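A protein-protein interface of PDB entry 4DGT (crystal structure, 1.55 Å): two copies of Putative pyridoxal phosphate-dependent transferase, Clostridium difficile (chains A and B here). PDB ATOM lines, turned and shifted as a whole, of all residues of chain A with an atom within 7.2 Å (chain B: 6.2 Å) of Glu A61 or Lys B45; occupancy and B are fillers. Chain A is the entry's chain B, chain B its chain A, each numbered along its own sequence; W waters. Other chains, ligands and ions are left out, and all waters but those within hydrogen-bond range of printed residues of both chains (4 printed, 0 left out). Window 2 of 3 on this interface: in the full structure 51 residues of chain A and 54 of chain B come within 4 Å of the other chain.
Water W4 lies within hydrogen-bond range of O of Asn B241, N of Tyr A63 and N of Ala B46.
Water W3 lies within hydrogen-bond range of OD1 of Asn B17, N of Gly A64 and NH2 of Arg A57.
Water W1 lies within hydrogen-bond range of the side-chain carboxylate of Glu A61 and the side-chain amino group of Lys B55.
Water W2 lies within hydrogen-bond range of the guanidinium group (NH2) of Arg A57 (2.8 Å), the backbone carbonyl oxygen (O) of Asn B17 (3.1 Å) and the backbone carbonyl oxygen (O) of Gly A64 (3.4 Å).
Leu A58 touches Lys B55.
Glu A61 touches Ile B51.
Ile A62 touches Val B12.
Ile A62 touches Met B42 (CG2 to O, 3.98 Å).
Ile A62 touches Phe B44 (CG1 to O, 3.8 Å).
CG1 of Ile A62 touches CA of Lys B45, 3.9 Å away.
Ile A62 touches Asn B241 (CG2 to ND2, 3.6 Å).
CE2 of Tyr A63 touches CB of Ala B46, at 3.7 Å.
CG1 of Ile B51 touches OH of Tyr A63, 3.8 Å away.
The backbone carbonyl oxygen (O) of Ile A62 lies within hydrogen-bond range of the guanidinium group (NH1) of Arg A57, 2.9 Å away.
O of Phe B44 is in hydrogen-bond range of ND2 of Asn B241, at 2.9 Å.
The side-chain amide nitrogen (ND2) of Asn B241 is in hydrogen-bond range of the backbone carbonyl oxygen (O) of Met B42 (2.9 Å).
The guanidinium group (NH1) of Arg A57 sits close to the side-chain amide oxygen (OE1) of Gln A60, 3.5 Å away.
The backbone carbonyl oxygen (O) of Leu A58 sits at hydrogen-bond distance from the side-chain hydroxyl (OH) of Tyr A63, 2.7 Å away.
OE2 of Glu B10 lies within salt-bridge range of NZ of Lys B45.
Printed residues of chain A within 4 Å of Ile B51: Glu A61 and Tyr A63.
Printed residues of chain B within 4 Å of Ile A62: Val B12 (3.3 Å), Asn B17 (3.3 Å), Met B42 (3.98 Å), Phe B44 (3.8 Å), Lys B45 (3.9 Å) and Asn B241 (3.6 Å).
Printed residues of chain A within 4 Å of Val B12: Ile A62 (3.3 Å).
Of the printed residues of chain A, Phe B44 touches Ile A62.
Of the printed residues of chain A, Met B42 touches Ile A62 (3.98 Å).
The nearest residue of chain B that does not touch Glu A61 is Phe B44 (4.7 Å).
The nearest residue of chain A that does not touch Lys B45 is Gln A60 (4.5 Å).
The nearest printed residue of chain A that does not touch Met B42 is Gly A64 (5.9 Å).
Of the 15 printed residues of chain B, 9 touch a printed residue of chain A.
Hydrophobic or aromatic side chains of chain B within 4 Å of the printed part of chain A: Val B12, Ala B46 and Ile B51.
Of the 9 printed residues of chain A, 6 touch a printed residue of chain B.
No position is printed for both chains.
Of the 15 pairs that touch across the chains among the printed residues, none has its exchanged pair printed and touching as well.
ND2 of Asn B17 sits close to NH2 of Arg A57, at 3.3 Å.
ND2 of Asn B17 sits at hydrogen-bond distance from O of Ile A62 (3.3 Å).
NZ of Lys B45 lies within salt-bridge range of OE1 of Glu A61, 3.3 Å away.
ND2 of Asn B17 is in hydrogen-bond range of OE1 of Gln A60, 2.7 Å away.
N of Ala B46 is in hydrogen-bond range of O of Glu A61, 3.0 Å away.
The backbone carbonyl oxygen (O) of Tyr A63 lies close to the backbone carbonyl oxygen (O) of Asn B241, at 3.4 Å.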
ATOM      1  N   ASN A  56      38.303  -1.958 -20.954  1.00  0.00           N
ATOM      2  CA  ASN A  56      38.686  -1.685 -22.324  1.00  0.00           C
ATOM      3  C   ASN A  56      38.168  -2.787 -23.237  1.00  0.00           C
ATOM      4  O   ASN A  56      37.654  -2.476 -24.317  1.00  0.00           O
ATOM      5  CB  ASN A  56      40.185  -1.466 -22.422  1.00  0.00           C
ATOM      6  CG  ASN A  56      40.595  -0.141 -21.726  1.00  0.00           C
ATOM      7  OD1 ASN A  56      39.881   0.861 -21.783  1.00  0.00           O
ATOM      8  ND2 ASN A  56      41.744  -0.154 -21.068  1.00  0.00           N
ATOM      9  N   ARG A  57      38.215  -4.026 -22.758  1.00  0.00           N
ATOM     10  CA  ARG A  57      37.642  -5.127 -23.520  1.00  0.00           C
ATOM     11  C   ARG A  57      36.110  -5.003 -23.690  1.00  0.00           C
ATOM     12  O   ARG A  57      35.548  -5.244 -24.788  1.00  0.00           O
ATOM     13  CB  ARG A  57      38.027  -6.494 -22.908  1.00  0.00           C
ATOM     14  CG  ARG A  57      37.553  -7.706 -23.693  1.00  0.00           C
ATOM     15  CD  ARG A  57      38.093  -7.676 -25.114  1.00  0.00           C
ATOM     16  NE  ARG A  57      37.577  -8.762 -25.944  1.00  0.00           N
ATOM     17  CZ  ARG A  57      36.420  -8.720 -26.592  1.00  0.00           C
ATOM     18  NH1 ARG A  57      35.580  -7.694 -26.424  1.00  0.00           N
ATOM     19  NH2 ARG A  57      36.066  -9.747 -27.368  1.00  0.00           N
ATOM     20  N   LEU A  58      35.459  -4.621 -22.600  1.00  0.00           N
ATOM     21  CA  LEU A  58      34.010  -4.446 -22.616  1.00  0.00           C
ATOM     22  C   LEU A  58      33.644  -3.421 -23.692  1.00  0.00           C
ATOM     23  O   LEU A  58      32.698  -3.611 -24.455  1.00  0.00           O
ATOM     24  CB  LEU A  58      33.551  -3.973 -21.255  1.00  0.00           C
ATOM     25  CG  LEU A  58      32.070  -4.109 -20.984  1.00  0.00           C
ATOM     26  CD1 LEU A  58      31.869  -4.330 -19.454  1.00  0.00           C
ATOM     27  CD2 LEU A  58      31.422  -2.888 -21.558  1.00  0.00           C
ATOM     28  N   GLU A  59      34.399  -2.308 -23.749  1.00  0.00           N
ATOM     29  CA  GLU A  59      34.060  -1.236 -24.671  1.00  0.00           C
ATOM     30  C   GLU A  59      34.293  -1.528 -26.155  1.00  0.00           C
ATOM     31  O   GLU A  59      33.850  -0.745 -27.005  1.00  0.00           O
ATOM     32  CB  GLU A  59      34.799   0.032 -24.234  1.00  0.00           C
ATOM     33  CG  GLU A  59      34.293   0.509 -22.864  1.00  0.00           C
ATOM     34  CD  GLU A  59      34.987   1.729 -22.358  1.00  0.00           C
ATOM     35  OE1 GLU A  59      36.115   2.039 -22.827  1.00  0.00           O
ATOM     36  OE2 GLU A  59      34.397   2.390 -21.462  1.00  0.00           O
ATOM     37  N   GLN A  60      34.878  -2.668 -26.496  1.00  0.00           N
ATOM     38  CA  GLN A  60      34.913  -3.097 -27.889  1.00  0.00           C
ATOM     39  C   GLN A  60      33.527  -3.520 -28.395  1.00  0.00           C
ATOM     40  O   GLN A  60      33.277  -3.518 -29.594  1.00  0.00           O
ATOM     41  CB  GLN A  60      35.939  -4.233 -28.075  1.00  0.00           C
ATOM     42  CG  GLN A  60      37.347  -3.770 -27.780  1.00  0.00           C
ATOM     43  CD  GLN A  60      38.382  -4.815 -27.973  1.00  0.00           C
ATOM     44  OE1 GLN A  60      38.067  -5.980 -28.124  1.00  0.00           O
ATOM     45  NE2 GLN A  60      39.648  -4.429 -27.896  1.00  0.00           N
ATOM     46  N   GLU A  61      32.684  -3.962 -27.458  1.00  0.00           N
ATOM     47  CA  GLU A  61      31.259  -4.210 -27.657  1.00  0.00           C
ATOM     48  C   GLU A  61      30.953  -5.438 -28.526  1.00  0.00           C
ATOM     49  O   GLU A  61      29.786  -5.656 -28.878  1.00  0.00           O
ATOM     50  CB  GLU A  61      30.511  -2.979 -28.164  1.00  0.00           C
ATOM     51  CG  GLU A  61      30.463  -1.902 -27.060  1.00  0.00           C
ATOM     52  CD  GLU A  61      29.719  -0.616 -27.380  1.00  0.00           C
ATOM     53  OE1 GLU A  61      29.417  -0.365 -28.552  1.00  0.00           O
ATOM     54  OE2 GLU A  61      29.432   0.140 -26.410  1.00  0.00           O
ATOM     55  N   ILE A  62      31.958  -6.266 -28.821  1.00  0.00           N
ATOM     56  CA  ILE A  62      31.767  -7.551 -29.557  1.00  0.00           C
ATOM     57  C   ILE A  62      32.427  -8.639 -28.728  1.00  0.00           C
ATOM     58  O   ILE A  62      33.590  -8.499 -28.382  1.00  0.00           O
ATOM     59  CB  ILE A  62      32.353  -7.531 -30.984  1.00  0.00           C
ATOM     60  CG1 ILE A  62      31.685  -6.425 -31.773  1.00  0.00           C
ATOM     61  CG2 ILE A  62      32.059  -8.875 -31.665  1.00  0.00           C
ATOM     62  CD1 ILE A  62      32.043  -6.332 -33.273  1.00  0.00           C
ATOM     63  N   TYR A  63      31.695  -9.720 -28.427  1.00  0.00           N
ATOM     64  CA  TYR A  63      32.152 -10.756 -27.540  1.00  0.00           C
ATOM     65  C   TYR A  63      32.130 -12.150 -28.177  1.00  0.00           C
ATOM     66  O   TYR A  63      31.514 -13.081 -27.665  1.00  0.00           O
ATOM     67  CB  TYR A  63      31.321 -10.782 -26.223  1.00  0.00           C
ATOM     68  CG  TYR A  63      31.163  -9.337 -25.680  1.00  0.00           C
ATOM     69  CD1 TYR A  63      32.267  -8.598 -25.246  1.00  0.00           C
ATOM     70  CD2 TYR A  63      29.894  -8.701 -25.705  1.00  0.00           C
ATOM     71  CE1 TYR A  63      32.111  -7.297 -24.833  1.00  0.00           C
ATOM     72  CE2 TYR A  63      29.744  -7.390 -25.291  1.00  0.00           C
ATOM     73  CZ  TYR A  63      30.877  -6.693 -24.832  1.00  0.00           C
ATOM     74  OH  TYR A  63      30.658  -5.343 -24.464  1.00  0.00           O
ATOM     75  N   GLY A  64      32.827 -12.261 -29.309  1.00  0.00           N
ATOM     76  CA  GLY A  64      32.834 -13.504 -30.066  1.00  0.00           C
ATOM     77  C   GLY A  64      33.944 -14.414 -29.652  1.00  0.00           C
ATOM     78  O   GLY A  64      34.607 -14.245 -28.612  1.00  0.00           O
ATOM     79  N   PHE B   8      22.892  -2.124 -37.493  1.00  0.00           N
ATOM     80  CA  PHE B   8      23.668  -3.264 -37.951  1.00  0.00           C
ATOM     81  C   PHE B   8      24.568  -2.931 -39.147  1.00  0.00           C
ATOM     82  O   PHE B   8      25.367  -3.745 -39.532  1.00  0.00           O
ATOM     83  CB  PHE B   8      22.708  -4.391 -38.389  1.00  0.00           C
ATOM     84  CG  PHE B   8      21.927  -4.978 -37.243  1.00  0.00           C
ATOM     85  CD1 PHE B   8      22.504  -5.878 -36.376  1.00  0.00           C
ATOM     86  CD2 PHE B   8      20.622  -4.587 -37.009  1.00  0.00           C
ATOM     87  CE1 PHE B   8      21.799  -6.372 -35.295  1.00  0.00           C
ATOM     88  CE2 PHE B   8      19.900  -5.084 -35.946  1.00  0.00           C
ATOM     89  CZ  PHE B   8      20.500  -5.961 -35.079  1.00  0.00           C
ATOM     90  N   GLU B  10      26.735  -0.546 -38.982  1.00  0.00           N
ATOM     91  CA  GLU B  10      27.950   0.006 -38.402  1.00  0.00           C
ATOM     92  C   GLU B  10      29.071  -1.001 -38.560  1.00  0.00           C
ATOM     93  O   GLU B  10      28.924  -2.156 -38.193  1.00  0.00           O
ATOM     94  CB  GLU B  10      27.724   0.309 -36.912  1.00  0.00           C
ATOM     95  CG  GLU B  10      28.996   0.479 -36.094  1.00  0.00           C
ATOM     96  CD  GLU B  10      28.739   1.019 -34.697  1.00  0.00           C
ATOM     97  OE1 GLU B  10      27.601   0.905 -34.208  1.00  0.00           O
ATOM     98  OE2 GLU B  10      29.679   1.566 -34.087  1.00  0.00           O
ATOM     99  N   VAL B  12      32.507  -2.452 -37.289  1.00  0.00           N
ATOM    100  CA  VAL B  12      33.300  -2.453 -36.085  1.00  0.00           C
ATOM    101  C   VAL B  12      34.621  -3.130 -36.404  1.00  0.00           C
ATOM    102  O   VAL B  12      34.647  -4.260 -36.866  1.00  0.00           O
ATOM    103  CB  VAL B  12      32.573  -3.216 -34.965  1.00  0.00           C
ATOM    104  CG1 VAL B  12      33.472  -3.383 -33.755  1.00  0.00           C
ATOM    105  CG2 VAL B  12      31.278  -2.506 -34.594  1.00  0.00           C
ATOM    106  N   ASN B  17      40.411  -7.003 -31.322  1.00  0.00           N
ATOM    107  CA  ASN B  17      39.311  -7.533 -30.549  1.00  0.00           C
ATOM    108  C   ASN B  17      39.584  -8.995 -30.181  1.00  0.00           C
ATOM    109  O   ASN B  17      38.651  -9.683 -29.769  1.00  0.00           O
ATOM    110  CB  ASN B  17      38.059  -7.390 -31.450  1.00  0.00           C
ATOM    111  CG  ASN B  17      36.771  -7.889 -30.852  1.00  0.00           C
ATOM    112  OD1 ASN B  17      36.063  -8.608 -31.519  1.00  0.00           O
ATOM    113  ND2 ASN B  17      36.414  -7.437 -29.658  1.00  0.00           N
ATOM    114  N   MET B  42      29.394 -13.352 -35.093  1.00  0.00           N
ATOM    115  CA  MET B  42      28.916 -12.231 -35.870  1.00  0.00           C
ATOM    116  C   MET B  42      29.817 -11.028 -35.801  1.00  0.00           C
ATOM    117  O   MET B  42      30.536 -10.784 -34.810  1.00  0.00           O
ATOM    118  CB  MET B  42      27.555 -11.719 -35.371  1.00  0.00           C
ATOM    119  CG  MET B  42      26.519 -12.728 -34.962  1.00  0.00           C
ATOM    120  SD  MET B  42      24.951 -11.863 -34.592  1.00  0.00           S
ATOM    121  CE  MET B  42      23.848 -13.189 -34.040  1.00  0.00           C
ATOM    122  N   ASP B  43      29.792 -10.254 -36.858  1.00  0.00           N
ATOM    123  CA  ASP B  43      30.464  -8.943 -36.901  1.00  0.00           C
ATOM    124  C   ASP B  43      29.533  -7.788 -36.516  1.00  0.00           C
ATOM    125  O   ASP B  43      29.550  -6.697 -37.122  1.00  0.00           O
ATOM    126  CB  ASP B  43      31.168  -8.746 -38.247  1.00  0.00           C
ATOM    127  CG  ASP B  43      32.588  -9.331 -38.248  1.00  0.00           C
ATOM    128  OD1 ASP B  43      32.778 -10.474 -37.758  1.00  0.00           O
ATOM    129  OD2 ASP B  43      33.534  -8.575 -38.647  1.00  0.00           O
ATOM    130  N   PHE B  44      28.752  -8.037 -35.485  1.00  0.00           N
ATOM    131  CA  PHE B  44      27.819  -7.086 -34.938  1.00  0.00           C
ATOM    132  C   PHE B  44      28.050  -6.927 -33.425  1.00  0.00           C
ATOM    133  O   PHE B  44      28.340  -7.891 -32.706  1.00  0.00           O
ATOM    134  CB  PHE B  44      26.376  -7.607 -35.109  1.00  0.00           C
ATOM    135  CG  PHE B  44      25.887  -7.702 -36.522  1.00  0.00           C
ATOM    136  CD1 PHE B  44      26.115  -6.731 -37.480  1.00  0.00           C
ATOM    137  CD2 PHE B  44      25.119  -8.767 -36.883  1.00  0.00           C
ATOM    138  CE1 PHE B  44      25.658  -6.866 -38.771  1.00  0.00           C
ATOM    139  CE2 PHE B  44      24.590  -8.852 -38.144  1.00  0.00           C
ATOM    140  CZ  PHE B  44      24.908  -7.946 -39.124  1.00  0.00           C
ATOM    141  N   LYS B  45      27.843  -5.707 -32.930  1.00  0.00           N
ATOM    142  CA  LYS B  45      27.882  -5.442 -31.513  1.00  0.00           C
ATOM    143  C   LYS B  45      26.779  -6.181 -30.803  1.00  0.00           C
ATOM    144  O   LYS B  45      25.693  -6.435 -31.378  1.00  0.00           O
ATOM    145  CB  LYS B  45      27.728  -3.927 -31.256  1.00  0.00           C
ATOM    146  CG  LYS B  45      28.837  -3.075 -31.850  1.00  0.00           C
ATOM    147  CD  LYS B  45      28.722  -1.585 -31.477  1.00  0.00           C
ATOM    148  CE  LYS B  45      30.111  -0.953 -31.526  1.00  0.00           C
ATOM    149  NZ  LYS B  45      30.130   0.546 -31.632  1.00  0.00           N
ATOM    150  N   ALA B  46      27.034  -6.559 -29.553  1.00  0.00           N
ATOM    151  CA  ALA B  46      26.025  -7.180 -28.701  1.00  0.00           C
ATOM    152  C   ALA B  46      24.947  -6.129 -28.464  1.00  0.00           C
ATOM    153  O   ALA B  46      25.193  -4.921 -28.541  1.00  0.00           O
ATOM    154  CB  ALA B  46      26.675  -7.628 -27.338  1.00  0.00           C
ATOM    155  N   ALA B  47      23.761  -6.618 -28.168  1.00  0.00           N
ATOM    156  CA  ALA B  47      22.605  -5.822 -27.805  1.00  0.00           C
ATOM    157  C   ALA B  47      22.960  -4.870 -26.666  1.00  0.00           C
ATOM    158  O   ALA B  47      23.757  -5.193 -25.774  1.00  0.00           O
ATOM    159  CB  ALA B  47      21.483  -6.768 -27.358  1.00  0.00           C
ATOM    160  N   ILE B  51      25.490  -5.279 -23.145  1.00  0.00           N
ATOM    161  CA  ILE B  51      26.627  -4.472 -22.869  1.00  0.00           C
ATOM    162  C   ILE B  51      26.435  -3.818 -21.487  1.00  0.00           C
ATOM    163  O   ILE B  51      27.366  -3.753 -20.695  1.00  0.00           O
ATOM    164  CB  ILE B  51      26.846  -3.390 -23.960  1.00  0.00           C
ATOM    165  CG1 ILE B  51      27.152  -4.050 -25.300  1.00  0.00           C
ATOM    166  CG2 ILE B  51      27.968  -2.428 -23.527  1.00  0.00           C
ATOM    167  CD1 ILE B  51      27.006  -3.039 -26.417  1.00  0.00           C
ATOM    168  N   LYS B  55      28.676  -3.965 -18.064  1.00  0.00           N
ATOM    169  CA  LYS B  55      29.159  -2.767 -17.370  1.00  0.00           C
ATOM    170  C   LYS B  55      28.764  -2.738 -15.900  1.00  0.00           C
ATOM    171  O   LYS B  55      29.570  -2.413 -15.058  1.00  0.00           O
ATOM    172  CB  LYS B  55      28.634  -1.470 -18.046  1.00  0.00           C
ATOM    173  CG  LYS B  55      29.238  -1.186 -19.408  1.00  0.00           C
ATOM    174  CD  LYS B  55      28.813   0.161 -19.969  1.00  0.00           C
ATOM    175  CE  LYS B  55      29.278   0.385 -21.410  1.00  0.00           C
ATOM    176  NZ  LYS B  55      28.525   1.538 -21.988  1.00  0.00           N
ATOM    177  N   PHE B 240      22.948 -14.263 -29.641  1.00  0.00           N
ATOM    178  CA  PHE B 240      23.274 -12.902 -29.245  1.00  0.00           C
ATOM    179  C   PHE B 240      24.747 -12.546 -29.467  1.00  0.00           C
ATOM    180  O   PHE B 240      25.179 -11.468 -29.049  1.00  0.00           O
ATOM    181  CB  PHE B 240      22.927 -12.705 -27.772  1.00  0.00           C
ATOM    182  CG  PHE B 240      21.469 -12.742 -27.524  1.00  0.00           C
ATOM    183  CD1 PHE B 240      20.672 -11.664 -27.897  1.00  0.00           C
ATOM    184  CD2 PHE B 240      20.846 -13.857 -26.973  1.00  0.00           C
ATOM    185  CE1 PHE B 240      19.300 -11.700 -27.723  1.00  0.00           C
ATOM    186  CE2 PHE B 240      19.449 -13.849 -26.782  1.00  0.00           C
ATOM    187  CZ  PHE B 240      18.710 -12.786 -27.144  1.00  0.00           C
ATOM    188  N   ASN B 241      25.522 -13.406 -30.125  1.00  0.00           N
ATOM    189  CA  ASN B 241      26.917 -13.143 -30.437  1.00  0.00           C
ATOM    190  C   ASN B 241      27.745 -13.007 -29.173  1.00  0.00           C
ATOM    191  O   ASN B 241      28.553 -12.051 -29.021  1.00  0.00           O
ATOM    192  CB  ASN B 241      27.092 -11.941 -31.402  1.00  0.00           C
ATOM    193  CG  ASN B 241      28.489 -11.926 -32.000  1.00  0.00           C
ATOM    194  OD1 ASN B 241      29.097 -12.978 -32.193  1.00  0.00           O
ATOM    195  ND2 ASN B 241      28.989 -10.725 -32.333  1.00  0.00           N
ATOM    196  N   TRP B 291      16.196  -6.648 -29.804  1.00  0.00           N
ATOM    197  CA  TRP B 291      17.416  -6.701 -30.649  1.00  0.00           C
ATOM    198  C   TRP B 291      17.384  -7.893 -31.567  1.00  0.00           C
ATOM    199  O   TRP B 291      17.692  -7.803 -32.759  1.00  0.00           O
ATOM    200  CB  TRP B 291      18.642  -6.718 -29.741  1.00  0.00           C
ATOM    201  CG  TRP B 291      19.925  -6.771 -30.505  1.00  0.00           C
ATOM    202  CD1 TRP B 291      20.677  -5.693 -30.950  1.00  0.00           C
ATOM    203  CD2 TRP B 291      20.611  -7.951 -30.982  1.00  0.00           C
ATOM    204  NE1 TRP B 291      21.802  -6.148 -31.620  1.00  0.00           N
ATOM    205  CE2 TRP B 291      21.780  -7.492 -31.709  1.00  0.00           C
ATOM    206  CE3 TRP B 291      20.339  -9.318 -30.941  1.00  0.00           C
ATOM    207  CZ2 TRP B 291      22.677  -8.406 -32.299  1.00  0.00           C
ATOM    208  CZ3 TRP B 291      21.210 -10.202 -31.566  1.00  0.00           C
ATOM    209  CH2 TRP B 291      22.338  -9.753 -32.258  1.00  0.00           C
HETATM  210  O   HOH W   1      30.933   0.208 -24.148  1.00  0.00           O
HETATM  211  O   HOH W   2      37.204 -12.054 -28.456  1.00  0.00           O
HETATM  212  O   HOH W   3      35.281 -10.914 -30.324  1.00  0.00           O
HETATM  213  O   HOH W   4      28.965  -9.429 -29.272  1.00  0.00           O
